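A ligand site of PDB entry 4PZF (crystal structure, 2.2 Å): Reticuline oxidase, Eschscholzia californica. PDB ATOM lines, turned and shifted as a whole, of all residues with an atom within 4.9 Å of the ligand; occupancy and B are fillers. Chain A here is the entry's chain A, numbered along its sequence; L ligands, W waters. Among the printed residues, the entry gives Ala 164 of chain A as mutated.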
ATOM      1  N   GLN A  59      32.554  28.939  33.118  1.00  0.00           N
ATOM      2  CA  GLN A  59      31.629  28.400  34.109  1.00  0.00           C
ATOM      3  C   GLN A  59      31.948  26.945  34.463  1.00  0.00           C
ATOM      4  O   GLN A  59      31.312  26.352  35.329  1.00  0.00           O
ATOM      5  CB  GLN A  59      30.191  28.508  33.599  1.00  0.00           C
ATOM      6  CG  GLN A  59      29.796  29.929  33.164  1.00  0.00           C
ATOM      7  CD  GLN A  59      29.661  30.898  34.330  1.00  0.00           C
ATOM      8  OE1 GLN A  59      29.867  30.546  35.492  1.00  0.00           O
ATOM      9  NE2 GLN A  59      29.294  32.139  34.017  1.00  0.00           N
ATOM     10  N   LEU A  99      32.654  32.059  19.663  1.00  0.00           N
ATOM     11  CA  LEU A  99      31.614  32.915  20.210  1.00  0.00           C
ATOM     12  C   LEU A  99      31.304  32.492  21.647  1.00  0.00           C
ATOM     13  O   LEU A  99      31.225  31.305  21.937  1.00  0.00           O
ATOM     14  CB  LEU A  99      30.345  32.843  19.363  1.00  0.00           C
ATOM     15  CG  LEU A  99      30.444  33.229  17.882  1.00  0.00           C
ATOM     16  CD1 LEU A  99      29.224  32.732  17.143  1.00  0.00           C
ATOM     17  CD2 LEU A  99      30.606  34.735  17.725  1.00  0.00           C
ATOM     18  N   ARG A 100      31.142  33.468  22.535  1.00  0.00           N
ATOM     19  CA  ARG A 100      30.743  33.149  23.904  1.00  0.00           C
ATOM     20  C   ARG A 100      29.657  34.077  24.410  1.00  0.00           C
ATOM     21  O   ARG A 100      29.795  35.303  24.354  1.00  0.00           O
ATOM     22  CB  ARG A 100      31.946  33.210  24.853  1.00  0.00           C
ATOM     23  CG  ARG A 100      31.581  32.842  26.294  1.00  0.00           C
ATOM     24  CD  ARG A 100      32.804  32.694  27.176  1.00  0.00           C
ATOM     25  NE  ARG A 100      33.436  33.979  27.485  1.00  0.00           N
ATOM     26  CZ  ARG A 100      34.557  34.108  28.185  1.00  0.00           C
ATOM     27  NH1 ARG A 100      35.059  35.311  28.411  1.00  0.00           N
ATOM     28  NH2 ARG A 100      35.183  33.041  28.654  1.00  0.00           N
ATOM     29  N   SER A 101      28.579  33.483  24.903  1.00  0.00           N
ATOM     30  CA  SER A 101      27.482  34.240  25.499  1.00  0.00           C
ATOM     31  C   SER A 101      27.545  34.156  27.012  1.00  0.00           C
ATOM     32  O   SER A 101      27.988  35.102  27.677  1.00  0.00           O
ATOM     33  CB  SER A 101      26.125  33.721  24.994  1.00  0.00           C
ATOM     34  OG  SER A 101      25.057  34.441  25.578  1.00  0.00           O
ATOM     35  N   GLY A 102      27.125  33.021  27.553  1.00  0.00           N
ATOM     36  CA  GLY A 102      27.147  32.808  28.988  1.00  0.00           C
ATOM     37  C   GLY A 102      28.326  31.961  29.442  1.00  0.00           C
ATOM     38  O   GLY A 102      28.654  31.933  30.635  1.00  0.00           O
ATOM     39  N   GLY A 103      28.955  31.268  28.499  1.00  0.00           N
ATOM     40  CA  GLY A 103      30.132  30.462  28.778  1.00  0.00           C
ATOM     41  C   GLY A 103      29.869  29.176  29.551  1.00  0.00           C
ATOM     42  O   GLY A 103      30.766  28.643  30.208  1.00  0.00           O
ATOM     43  N   HIS A 104      28.641  28.669  29.453  1.00  0.00           N
ATOM     44  CA  HIS A 104      28.254  27.486  30.213  1.00  0.00           C
ATOM     45  C   HIS A 104      28.493  26.175  29.487  1.00  0.00           C
ATOM     46  O   HIS A 104      28.061  25.119  29.957  1.00  0.00           O
ATOM     47  CB  HIS A 104      26.776  27.575  30.612  1.00  0.00           C
ATOM     48  CG  HIS A 104      26.558  28.147  31.979  1.00  0.00           C
ATOM     49  ND1 HIS A 104      26.451  27.357  33.107  1.00  0.00           N
ATOM     50  CD2 HIS A 104      26.452  29.421  32.399  1.00  0.00           C
ATOM     51  CE1 HIS A 104      26.279  28.132  34.164  1.00  0.00           C
ATOM     52  NE2 HIS A 104      26.273  29.396  33.761  1.00  0.00           N
ATOM     53  N   SER A 105      29.179  26.239  28.354  1.00  0.00           N
ATOM     54  CA  SER A 105      29.507  25.046  27.579  1.00  0.00           C
ATOM     55  C   SER A 105      30.109  23.967  28.468  1.00  0.00           C
ATOM     56  O   SER A 105      31.136  24.192  29.122  1.00  0.00           O
ATOM     57  CB  SER A 105      30.454  25.382  26.440  1.00  0.00           C
ATOM     58  OG  SER A 105      30.908  24.201  25.792  1.00  0.00           O
ATOM     59  N   TYR A 106      29.464  22.808  28.507  1.00  0.00           N
ATOM     60  CA  TYR A 106      29.925  21.699  29.343  1.00  0.00           C
ATOM     61  C   TYR A 106      31.349  21.287  28.983  1.00  0.00           C
ATOM     62  O   TYR A 106      32.098  20.806  29.837  1.00  0.00           O
ATOM     63  CB  TYR A 106      28.975  20.512  29.195  1.00  0.00           C
ATOM     64  CG  TYR A 106      27.644  20.684  29.915  1.00  0.00           C
ATOM     65  CD1 TYR A 106      27.466  21.707  30.840  1.00  0.00           C
ATOM     66  CD2 TYR A 106      26.594  19.817  29.673  1.00  0.00           C
ATOM     67  CE1 TYR A 106      26.261  21.858  31.503  1.00  0.00           C
ATOM     68  CE2 TYR A 106      25.390  19.961  30.329  1.00  0.00           C
ATOM     69  CZ  TYR A 106      25.227  20.979  31.247  1.00  0.00           C
ATOM     70  OH  TYR A 106      24.029  21.129  31.897  1.00  0.00           O
ATOM     71  N   LEU A 109      33.568  24.756  24.882  1.00  0.00           N
ATOM     72  CA  LEU A 109      33.738  24.949  23.443  1.00  0.00           C
ATOM     73  C   LEU A 109      33.603  26.409  23.014  1.00  0.00           C
ATOM     74  O   LEU A 109      33.842  26.739  21.856  1.00  0.00           O
ATOM     75  CB  LEU A 109      32.736  24.098  22.664  1.00  0.00           C
ATOM     76  CG  LEU A 109      32.824  22.579  22.867  1.00  0.00           C
ATOM     77  CD1 LEU A 109      31.842  21.853  21.973  1.00  0.00           C
ATOM     78  CD2 LEU A 109      34.249  22.081  22.613  1.00  0.00           C
ATOM     79  N   SER A 110      33.197  27.278  23.929  1.00  0.00           N
ATOM     80  CA  SER A 110      32.991  28.677  23.596  1.00  0.00           C
ATOM     81  C   SER A 110      34.250  29.511  23.838  1.00  0.00           C
ATOM     82  O   SER A 110      34.319  30.655  23.415  1.00  0.00           O
ATOM     83  CB  SER A 110      31.835  29.270  24.386  1.00  0.00           C
ATOM     84  OG  SER A 110      32.011  29.077  25.785  1.00  0.00           O
ATOM     85  N   LEU A 122      30.115  38.232  24.035  1.00  0.00           N
ATOM     86  CA  LEU A 122      28.898  38.981  23.723  1.00  0.00           C
ATOM     87  C   LEU A 122      28.238  39.634  24.937  1.00  0.00           C
ATOM     88  O   LEU A 122      27.088  40.066  24.856  1.00  0.00           O
ATOM     89  CB  LEU A 122      27.896  38.044  23.050  1.00  0.00           C
ATOM     90  CG  LEU A 122      28.436  37.338  21.796  1.00  0.00           C
ATOM     91  CD1 LEU A 122      27.551  36.170  21.390  1.00  0.00           C
ATOM     92  CD2 LEU A 122      28.572  38.337  20.657  1.00  0.00           C
ATOM     93  N   SER A 141      21.864  38.339  22.175  1.00  0.00           N
ATOM     94  CA  SER A 141      22.326  36.984  22.479  1.00  0.00           C
ATOM     95  C   SER A 141      23.323  36.892  23.627  1.00  0.00           C
ATOM     96  O   SER A 141      23.707  35.794  24.026  1.00  0.00           O
ATOM     97  CB  SER A 141      22.942  36.363  21.237  1.00  0.00           C
ATOM     98  OG  SER A 141      24.088  37.094  20.803  1.00  0.00           O
ATOM     99  N   ALA A 164      15.773  27.225  30.997  1.00  0.00           N
ATOM    100  CA  ALA A 164      16.461  26.645  32.152  1.00  0.00           C
ATOM    101  C   ALA A 164      16.294  27.447  33.445  1.00  0.00           C
ATOM    102  O   ALA A 164      15.904  28.614  33.428  1.00  0.00           O
ATOM    103  CB  ALA A 164      17.934  26.496  31.844  1.00  0.00           C
ATOM    104  N   TRP A 165      16.605  26.794  34.562  1.00  0.00           N
ATOM    105  CA  TRP A 165      16.549  27.447  35.859  1.00  0.00           C
ATOM    106  C   TRP A 165      17.854  28.176  36.161  1.00  0.00           C
ATOM    107  O   TRP A 165      17.872  29.133  36.942  1.00  0.00           O
ATOM    108  CB  TRP A 165      16.250  26.423  36.965  1.00  0.00           C
ATOM    109  CG  TRP A 165      17.272  25.333  37.090  1.00  0.00           C
ATOM    110  CD1 TRP A 165      17.208  24.083  36.538  1.00  0.00           C
ATOM    111  CD2 TRP A 165      18.518  25.389  37.802  1.00  0.00           C
ATOM    112  NE1 TRP A 165      18.333  23.365  36.860  1.00  0.00           N
ATOM    113  CE2 TRP A 165      19.156  24.141  37.642  1.00  0.00           C
ATOM    114  CE3 TRP A 165      19.159  26.369  38.569  1.00  0.00           C
ATOM    115  CZ2 TRP A 165      20.397  23.846  38.212  1.00  0.00           C
ATOM    116  CZ3 TRP A 165      20.384  26.081  39.130  1.00  0.00           C
ATOM    117  CH2 TRP A 165      20.994  24.830  38.953  1.00  0.00           C
ATOM    118  N   CYS A 166      18.944  27.722  35.550  1.00  0.00           N
ATOM    119  CA  CYS A 166      20.259  28.344  35.703  1.00  0.00           C
ATOM    120  C   CYS A 166      20.242  29.763  35.133  1.00  0.00           C
ATOM    121  O   CYS A 166      20.199  29.946  33.917  1.00  0.00           O
ATOM    122  CB  CYS A 166      21.330  27.515  35.001  1.00  0.00           C
ATOM    123  SG  CYS A 166      21.490  25.788  35.541  1.00  0.00           S
ATOM    124  N   THR A 168      22.500  32.169  34.961  1.00  0.00           N
ATOM    125  CA  THR A 168      23.696  32.723  34.328  1.00  0.00           C
ATOM    126  C   THR A 168      23.971  32.087  32.966  1.00  0.00           C
ATOM    127  O   THR A 168      24.926  32.441  32.294  1.00  0.00           O
ATOM    128  CB  THR A 168      24.945  32.558  35.217  1.00  0.00           C
ATOM    129  OG1 THR A 168      25.193  31.177  35.450  1.00  0.00           O
ATOM    130  CG2 THR A 168      24.746  33.270  36.542  1.00  0.00           C
ATOM    131  N   VAL A 169      23.113  31.140  32.579  1.00  0.00           N
ATOM    132  CA  VAL A 169      23.183  30.555  31.243  1.00  0.00           C
ATOM    133  C   VAL A 169      22.807  31.596  30.201  1.00  0.00           C
ATOM    134  O   VAL A 169      21.816  32.318  30.355  1.00  0.00           O
ATOM    135  CB  VAL A 169      22.257  29.326  31.129  1.00  0.00           C
ATOM    136  CG1 VAL A 169      21.988  28.989  29.660  1.00  0.00           C
ATOM    137  CG2 VAL A 169      22.853  28.139  31.853  1.00  0.00           C
ATOM    138  N   GLY A 170      23.616  31.716  29.149  1.00  0.00           N
ATOM    139  CA  GLY A 170      23.350  32.683  28.102  1.00  0.00           C
ATOM    140  C   GLY A 170      22.332  32.207  27.084  1.00  0.00           C
ATOM    141  O   GLY A 170      22.304  31.031  26.725  1.00  0.00           O
ATOM    142  N   THR A 171      21.486  33.116  26.610  1.00  0.00           N
ATOM    143  CA  THR A 171      20.492  32.803  25.599  1.00  0.00           C
ATOM    144  C   THR A 171      21.141  32.389  24.275  1.00  0.00           C
ATOM    145  O   THR A 171      20.545  31.666  23.479  1.00  0.00           O
ATOM    146  CB  THR A 171      19.554  33.984  25.334  1.00  0.00           C
ATOM    147  OG1 THR A 171      20.333  35.127  24.940  1.00  0.00           O
ATOM    148  CG2 THR A 171      18.742  34.334  26.578  1.00  0.00           C
ATOM    149  N   GLY A 172      22.364  32.862  24.056  1.00  0.00           N
ATOM    150  CA  GLY A 172      23.098  32.581  22.842  1.00  0.00           C
ATOM    151  C   GLY A 172      23.277  31.093  22.588  1.00  0.00           C
ATOM    152  O   GLY A 172      22.914  30.587  21.530  1.00  0.00           O
ATOM    153  N   GLY A 173      23.838  30.393  23.567  1.00  0.00           N
ATOM    154  CA  GLY A 173      24.052  28.969  23.442  1.00  0.00           C
ATOM    155  C   GLY A 173      22.819  28.163  23.808  1.00  0.00           C
ATOM    156  O   GLY A 173      22.529  27.148  23.171  1.00  0.00           O
ATOM    157  N   HIS A 174      22.091  28.620  24.821  1.00  0.00           N
ATOM    158  CA  HIS A 174      20.940  27.896  25.350  1.00  0.00           C
ATOM    159  C   HIS A 174      19.845  27.681  24.305  1.00  0.00           C
ATOM    160  O   HIS A 174      19.427  26.558  24.054  1.00  0.00           O
ATOM    161  CB  HIS A 174      20.354  28.640  26.541  1.00  0.00           C
ATOM    162  CG  HIS A 174      19.310  27.866  27.289  1.00  0.00           C
ATOM    163  ND1 HIS A 174      19.578  26.670  27.917  1.00  0.00           N
ATOM    164  CD2 HIS A 174      17.992  28.121  27.511  1.00  0.00           C
ATOM    165  CE1 HIS A 174      18.481  26.216  28.492  1.00  0.00           C
ATOM    166  NE2 HIS A 174      17.509  27.084  28.260  1.00  0.00           N
ATOM    167  N   SER A 176      20.071  28.274  21.098  1.00  0.00           N
ATOM    168  CA  SER A 176      20.674  27.659  19.922  1.00  0.00           C
ATOM    169  C   SER A 176      20.649  26.132  19.980  1.00  0.00           C
ATOM    170  O   SER A 176      20.660  25.470  18.936  1.00  0.00           O
ATOM    171  CB  SER A 176      22.124  28.126  19.751  1.00  0.00           C
ATOM    172  OG  SER A 176      22.184  29.481  19.337  1.00  0.00           O
ATOM    173  N   GLY A 179      16.889  24.280  24.773  1.00  0.00           N
ATOM    174  CA  GLY A 179      16.544  24.985  25.990  1.00  0.00           C
ATOM    175  C   GLY A 179      15.389  24.359  26.752  1.00  0.00           C
ATOM    176  O   GLY A 179      14.238  24.743  26.560  1.00  0.00           O
ATOM    177  N   PHE A 180      15.710  23.407  27.616  1.00  0.00           N
ATOM    178  CA  PHE A 180      14.698  22.687  28.386  1.00  0.00           C
ATOM    179  C   PHE A 180      14.618  23.236  29.818  1.00  0.00           C
ATOM    180  O   PHE A 180      15.641  23.543  30.430  1.00  0.00           O
ATOM    181  CB  PHE A 180      15.020  21.191  28.402  1.00  0.00           C
ATOM    182  CG  PHE A 180      13.987  20.358  29.113  1.00  0.00           C
ATOM    183  CD1 PHE A 180      12.871  19.895  28.430  1.00  0.00           C
ATOM    184  CD2 PHE A 180      14.138  20.023  30.438  1.00  0.00           C
ATOM    185  CE1 PHE A 180      11.922  19.123  29.061  1.00  0.00           C
ATOM    186  CE2 PHE A 180      13.191  19.249  31.087  1.00  0.00           C
ATOM    187  CZ  PHE A 180      12.085  18.806  30.399  1.00  0.00           C
ATOM    188  N   GLY A 225      24.794  25.761  18.987  1.00  0.00           N
ATOM    189  CA  GLY A 225      25.493  27.025  18.846  1.00  0.00           C
ATOM    190  C   GLY A 225      26.848  26.883  18.187  1.00  0.00           C
ATOM    191  O   GLY A 225      27.450  25.810  18.201  1.00  0.00           O
ATOM    192  N   GLY A 226      27.334  27.977  17.613  1.00  0.00           N
ATOM    193  CA  GLY A 226      28.657  28.035  17.015  1.00  0.00           C
ATOM    194  C   GLY A 226      28.781  27.270  15.718  1.00  0.00           C
ATOM    195  O   GLY A 226      29.858  26.761  15.398  1.00  0.00           O
ATOM    196  N   GLY A 229      26.612  30.696  12.329  1.00  0.00           N
ATOM    197  CA  GLY A 229      26.929  32.113  12.309  1.00  0.00           C
ATOM    198  C   GLY A 229      26.734  32.620  13.719  1.00  0.00           C
ATOM    199  O   GLY A 229      26.543  31.841  14.644  1.00  0.00           O
ATOM    200  N   ALA A 230      26.775  33.938  13.884  1.00  0.00           N
ATOM    201  CA  ALA A 230      26.589  34.519  15.204  1.00  0.00           C
ATOM    202  C   ALA A 230      25.185  35.073  15.358  1.00  0.00           C
ATOM    203  O   ALA A 230      24.809  36.012  14.659  1.00  0.00           O
ATOM    204  CB  ALA A 230      27.622  35.608  15.457  1.00  0.00           C
ATOM    205  N   ILE A 231      24.406  34.472  16.251  1.00  0.00           N
ATOM    206  CA  ILE A 231      23.095  35.030  16.580  1.00  0.00           C
ATOM    207  C   ILE A 231      23.300  36.359  17.278  1.00  0.00           C
ATOM    208  O   ILE A 231      23.962  36.429  18.310  1.00  0.00           O
ATOM    209  CB  ILE A 231      22.286  34.098  17.509  1.00  0.00           C
ATOM    210  CG1 ILE A 231      22.038  32.743  16.845  1.00  0.00           C
ATOM    211  CG2 ILE A 231      20.970  34.757  17.892  1.00  0.00           C
ATOM    212  CD1 ILE A 231      20.982  32.780  15.759  1.00  0.00           C
ATOM    213  N   TYR A 456      21.749  15.154  23.947  1.00  0.00           N
ATOM    214  CA  TYR A 456      21.129  16.473  23.859  1.00  0.00           C
ATOM    215  C   TYR A 456      22.243  17.495  23.609  1.00  0.00           C
ATOM    216  O   TYR A 456      23.199  17.561  24.377  1.00  0.00           O
ATOM    217  CB  TYR A 456      20.362  16.757  25.151  1.00  0.00           C
ATOM    218  CG  TYR A 456      19.807  18.161  25.337  1.00  0.00           C
ATOM    219  CD1 TYR A 456      19.440  18.949  24.257  1.00  0.00           C
ATOM    220  CD2 TYR A 456      19.656  18.675  26.617  1.00  0.00           C
ATOM    221  CE1 TYR A 456      18.935  20.222  24.459  1.00  0.00           C
ATOM    222  CE2 TYR A 456      19.161  19.938  26.817  1.00  0.00           C
ATOM    223  CZ  TYR A 456      18.797  20.708  25.741  1.00  0.00           C
ATOM    224  OH  TYR A 456      18.295  21.972  25.953  1.00  0.00           O
ATOM    225  N   ASN A 458      22.765  20.616  23.919  1.00  0.00           N
ATOM    226  CA  ASN A 458      23.129  21.531  24.999  1.00  0.00           C
ATOM    227  C   ASN A 458      23.869  20.795  26.107  1.00  0.00           C
ATOM    228  O   ASN A 458      24.533  21.409  26.944  1.00  0.00           O
ATOM    229  CB  ASN A 458      21.892  22.227  25.562  1.00  0.00           C
ATOM    230  CG  ASN A 458      21.614  23.559  24.876  1.00  0.00           C
ATOM    231  OD1 ASN A 458      22.529  24.208  24.383  1.00  0.00           O
ATOM    232  ND2 ASN A 458      20.345  23.951  24.844  1.00  0.00           N
ATOM    233  N   HIS A 459      23.734  19.475  26.116  1.00  0.00           N
ATOM    234  CA  HIS A 459      24.574  18.629  26.948  1.00  0.00           C
ATOM    235  C   HIS A 459      25.695  18.053  26.104  1.00  0.00           C
ATOM    236  O   HIS A 459      25.885  16.831  26.069  1.00  0.00           O
ATOM    237  CB  HIS A 459      23.742  17.510  27.588  1.00  0.00           C
ATOM    238  CG  HIS A 459      23.130  17.882  28.904  1.00  0.00           C
ATOM    239  ND1 HIS A 459      23.482  17.256  30.074  1.00  0.00           N
ATOM    240  CD2 HIS A 459      22.222  18.829  29.231  1.00  0.00           C
ATOM    241  CE1 HIS A 459      22.803  17.787  31.076  1.00  0.00           C
ATOM    242  NE2 HIS A 459      22.024  18.751  30.587  1.00  0.00           N
ATOM    243  N   HIS A 512      33.512  23.490  15.292  1.00  0.00           N
ATOM    244  CA  HIS A 512      34.062  22.998  16.548  1.00  0.00           C
ATOM    245  C   HIS A 512      34.006  21.459  16.466  1.00  0.00           C
ATOM    246  O   HIS A 512      33.491  20.937  15.486  1.00  0.00           O
ATOM    247  CB  HIS A 512      33.313  23.593  17.748  1.00  0.00           C
ATOM    248  CG  HIS A 512      31.869  23.184  17.845  1.00  0.00           C
ATOM    249  ND1 HIS A 512      31.484  21.914  18.197  1.00  0.00           N
ATOM    250  CD2 HIS A 512      30.737  23.897  17.675  1.00  0.00           C
ATOM    251  CE1 HIS A 512      30.160  21.854  18.224  1.00  0.00           C
ATOM    252  NE2 HIS A 512      29.689  23.041  17.906  1.00  0.00           N
HETATM  253  P1  LIG L   1      28.406  29.280  25.836  1.00  0.00           P
HETATM  254  O1  LIG L   1      29.553  28.413  26.289  1.00  0.00           O
HETATM  255  O2  LIG L   1      28.493  30.778  25.922  1.00  0.00           O
HETATM  256  O3  LIG L   1      28.008  28.823  24.337  1.00  0.00           O
HETATM  257  C1  LIG L   1      27.787  27.444  24.041  1.00  0.00           C
HETATM  258  C2  LIG L   1      27.881  27.227  22.539  1.00  0.00           C
HETATM  259  O4  LIG L   1      26.994  28.126  21.863  1.00  0.00           O
HETATM  260  C3  LIG L   1      29.281  27.527  22.036  1.00  0.00           C
HETATM  261  O5  LIG L   1      29.595  26.653  20.963  1.00  0.00           O
HETATM  262  C4  LIG L   1      29.188  28.938  21.505  1.00  0.00           C
HETATM  263  O6  LIG L   1      30.136  29.152  20.466  1.00  0.00           O
HETATM  264  C5  LIG L   1      27.747  28.994  21.005  1.00  0.00           C
HETATM  265  N1  LIG L   1      27.173  30.363  21.078  1.00  0.00           N
HETATM  266  C6  LIG L   1      27.115  31.157  22.164  1.00  0.00           C
HETATM  267  N2  LIG L   1      26.522  32.339  21.859  1.00  0.00           N
HETATM  268  C7  LIG L   1      26.194  32.312  20.548  1.00  0.00           C
HETATM  269  C8  LIG L   1      25.550  33.233  19.585  1.00  0.00           C
HETATM  270  N3  LIG L   1      25.120  34.457  19.956  1.00  0.00           N
HETATM  271  N4  LIG L   1      25.400  32.813  18.313  1.00  0.00           N
HETATM  272  C9  LIG L   1      25.821  31.595  17.919  1.00  0.00           C
HETATM  273  N5  LIG L   1      26.416  30.705  18.738  1.00  0.00           N
HETATM  274  C10 LIG L   1      26.636  31.001  20.037  1.00  0.00           C
HETATM  275  N6  LIG L   1      20.455  23.259  29.613  1.00  0.00           N
HETATM  276  C11 LIG L   1      19.134  23.001  29.586  1.00  0.00           C
HETATM  277  O7  LIG L   1      18.604  22.698  28.488  1.00  0.00           O
HETATM  278  N7  LIG L   1      18.347  23.064  30.683  1.00  0.00           N
HETATM  279  C12 LIG L   1      18.843  23.376  31.884  1.00  0.00           C
HETATM  280  O8  LIG L   1      18.097  23.435  32.891  1.00  0.00           O
HETATM  281  C13 LIG L   1      20.283  23.667  32.001  1.00  0.00           C
HETATM  282  N8  LIG L   1      20.859  24.000  33.164  1.00  0.00           N
HETATM  283  C14 LIG L   1      22.124  24.424  33.209  1.00  0.00           C
HETATM  284  C15 LIG L   1      22.627  24.938  34.388  1.00  0.00           C
HETATM  285  C16 LIG L   1      23.937  25.392  34.440  1.00  0.00           C
HETATM  286  C17 LIG L   1      24.476  25.926  35.736  1.00  0.00           C
HETATM  287  C18 LIG L   1      24.813  25.331  33.238  1.00  0.00           C
HETATM  288  C19 LIG L   1      26.244  25.831  33.323  1.00  0.00           C
HETATM  289  C20 LIG L   1      24.317  24.817  32.047  1.00  0.00           C
HETATM  290  C21 LIG L   1      22.993  24.360  31.996  1.00  0.00           C
HETATM  291  N9  LIG L   1      22.462  23.843  30.801  1.00  0.00           N
HETATM  292  C22 LIG L   1      21.076  23.579  30.754  1.00  0.00           C
HETATM  293  C23 LIG L   1      23.278  23.757  29.601  1.00  0.00           C
HETATM  294  C24 LIG L   1      23.074  24.974  28.697  1.00  0.00           C
HETATM  295  O9  LIG L   1      21.797  24.912  28.074  1.00  0.00           O
HETATM  296  C25 LIG L   1      24.140  24.964  27.624  1.00  0.00           C
HETATM  297  O10 LIG L   1      25.415  24.935  28.271  1.00  0.00           O
HETATM  298  C26 LIG L   1      24.002  26.220  26.779  1.00  0.00           C
HETATM  299  O11 LIG L   1      24.453  25.956  25.452  1.00  0.00           O
HETATM  300  C27 LIG L   1      24.805  27.338  27.430  1.00  0.00           C
HETATM  301  O12 LIG L   1      24.697  28.539  26.664  1.00  0.00           O
HETATM  302  P2  LIG L   1      25.809  29.667  26.934  1.00  0.00           P
HETATM  303  O13 LIG L   1      25.643  30.742  25.894  1.00  0.00           O
HETATM  304  O14 LIG L   1      25.836  29.988  28.406  1.00  0.00           O
HETATM  305  O15 LIG L   1      27.092  28.759  26.604  1.00  0.00           O
HETATM  306  O   HOH W   1      32.077  29.358  18.353  1.00  0.00           O
HETATM  307  O   HOH W   2      26.877  22.651  27.171  1.00  0.00           O
HETATM  308  O   HOH W   3      26.565  23.923  24.748  1.00  0.00           O
HETATM  309  O   HOH W   4      25.616  29.324  15.339  1.00  0.00           O
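O15 of the ligand lies within hydrogen-bond range of N of His 104 (3.2 Å).
An oxygen (O10) of the ligand sits at hydrogen-bond distance from the backbone carbonyl oxygen (O) of His 104 (3.1 Å).
C19 of the ligand is covalently linked to ND1 of His 104, 1.6 Å away.
The side-chain sulfur of Cys 166 is covalently linked to a carbon (C15) of the ligand.
An oxygen (O1) of the ligand sits at hydrogen-bond distance from the side-chain hydroxyl (OG) of Ser 110, at 2.6 Å.
The side-chain hydroxyl (OH) of Tyr 456 sits at hydrogen-bond distance from an oxygen (O7) of the ligand (2.7 Å).
N of Gly 103 lies within hydrogen-bond range of O2 of the ligand, at 2.7 Å.
The backbone NH of Phe 180 is in hydrogen-bond range of an oxygen (O7) of the ligand.
A nitrogen (N7) of the ligand is in hydrogen-bond range of the backbone carbonyl oxygen (O) of Phe 180, at 2.8 Å.
OD1 of Asn 458 is in hydrogen-bond range of O11 of the ligand, 2.8 Å away.
N of Ile 231 sits at hydrogen-bond distance from N4 of the ligand, at 2.8 Å.
O of Ile 231 sits at hydrogen-bond distance from N3 of the ligand (2.8 Å).
The backbone carbonyl oxygen of Leu 99 sits at hydrogen-bond distance from an oxygen (O6) of the ligand.
The backbone NH (N) of His 174 lies within hydrogen-bond range of an oxygen (O12) of the ligand (3.2 Å).
An oxygen (O9) of the ligand sits at hydrogen-bond distance from a ring nitrogen (ND1) of His 174, at 2.8 Å.
An oxygen (O2) of the ligand sits at hydrogen-bond distance from the backbone NH of Ser 101, at 2.9 Å.
An oxygen (O14) of the ligand lies within hydrogen-bond range of the backbone NH (N) of Gly 170.
N3 of the ligand sits at hydrogen-bond distance from OG of Ser 141 (3.0 Å).
The backbone NH of Gly 173 lies within hydrogen-bond range of an oxygen (O13) of the ligand (3.0 Å).
An oxygen (O11) of the ligand sits close to the backbone carbonyl oxygen (O) of Gly 173.
N of Ser 105 lies within hydrogen-bond range of O1 of the ligand.
The backbone NH (N) of Gly 226 sits at hydrogen-bond distance from a nitrogen (N5) of the ligand.
An oxygen (O2) of the ligand sits at hydrogen-bond distance from the backbone NH (N) of Gly 102 (3.1 Å).
The side-chain hydroxyl (OH) of Tyr 456 sits at hydrogen-bond distance from the backbone NH (N) of Phe 180 (3.4 Å).
N of Gln 59 lies close to O of Gly 103.
OD1 of Asn 458 sits close to O of Gly 173, at 3.2 Å.
ND2 of Asn 458 sits close to N of Gly 179, 3.5 Å away.
The backbone carbonyl oxygen of Ile 231 lies within hydrogen-bond range of the side-chain hydroxyl of Ser 141 (2.6 Å).
The backbone NH (N) of Gly 172 lies within hydrogen-bond range of the side-chain hydroxyl (OG) of Ser 101 (3.5 Å).
NE2 of Gln 59 sits close to O of Gly 102 (3.4 Å).
N of Leu 122 lies within hydrogen-bond range of O of Arg 100, at 3.0 Å.
OH of Tyr 106 sits close to N9 of the ligand (3.3 Å).
Arg 100 touches the ligand.
Leu 122 touches the ligand (CD1 to N3, 3.3 Å).
Ala 164 touches the ligand.
Trp 165 touches the ligand (CD1 to O8, 3.8 Å).
CG2 of Val 169 touches C20 of the ligand, 3.6 Å away.
Gly 172 touches the ligand (C to N2, 3.6 Å).
Gly 179 touches the ligand (CA to O7, 3.96 Å).
Gly 225 touches the ligand.
Gly 229 touches the ligand.
C of Ala 230 touches N4 of the ligand, 3.7 Å away.
Hydrophobic or aromatic side chains within 4 Å of the ligand: Leu 99, His 104, Tyr 106, Leu 122, Ala 164, Trp 165, Val 169, His 174, Phe 180, Ile 231 and Tyr 456.
Of the 35 residues printed, 28 come within 4 Å of the ligand.
Water W1 bridges O6 of the ligand (2.9 Å) and N of Leu 99 (3.1 Å).
Water W2 lies within hydrogen-bond range of the backbone carbonyl oxygen of Asn 458 (2.7 Å), the backbone NH of Tyr 106 (2.9 Å) and an oxygen (O10) of the ligand (2.9 Å).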
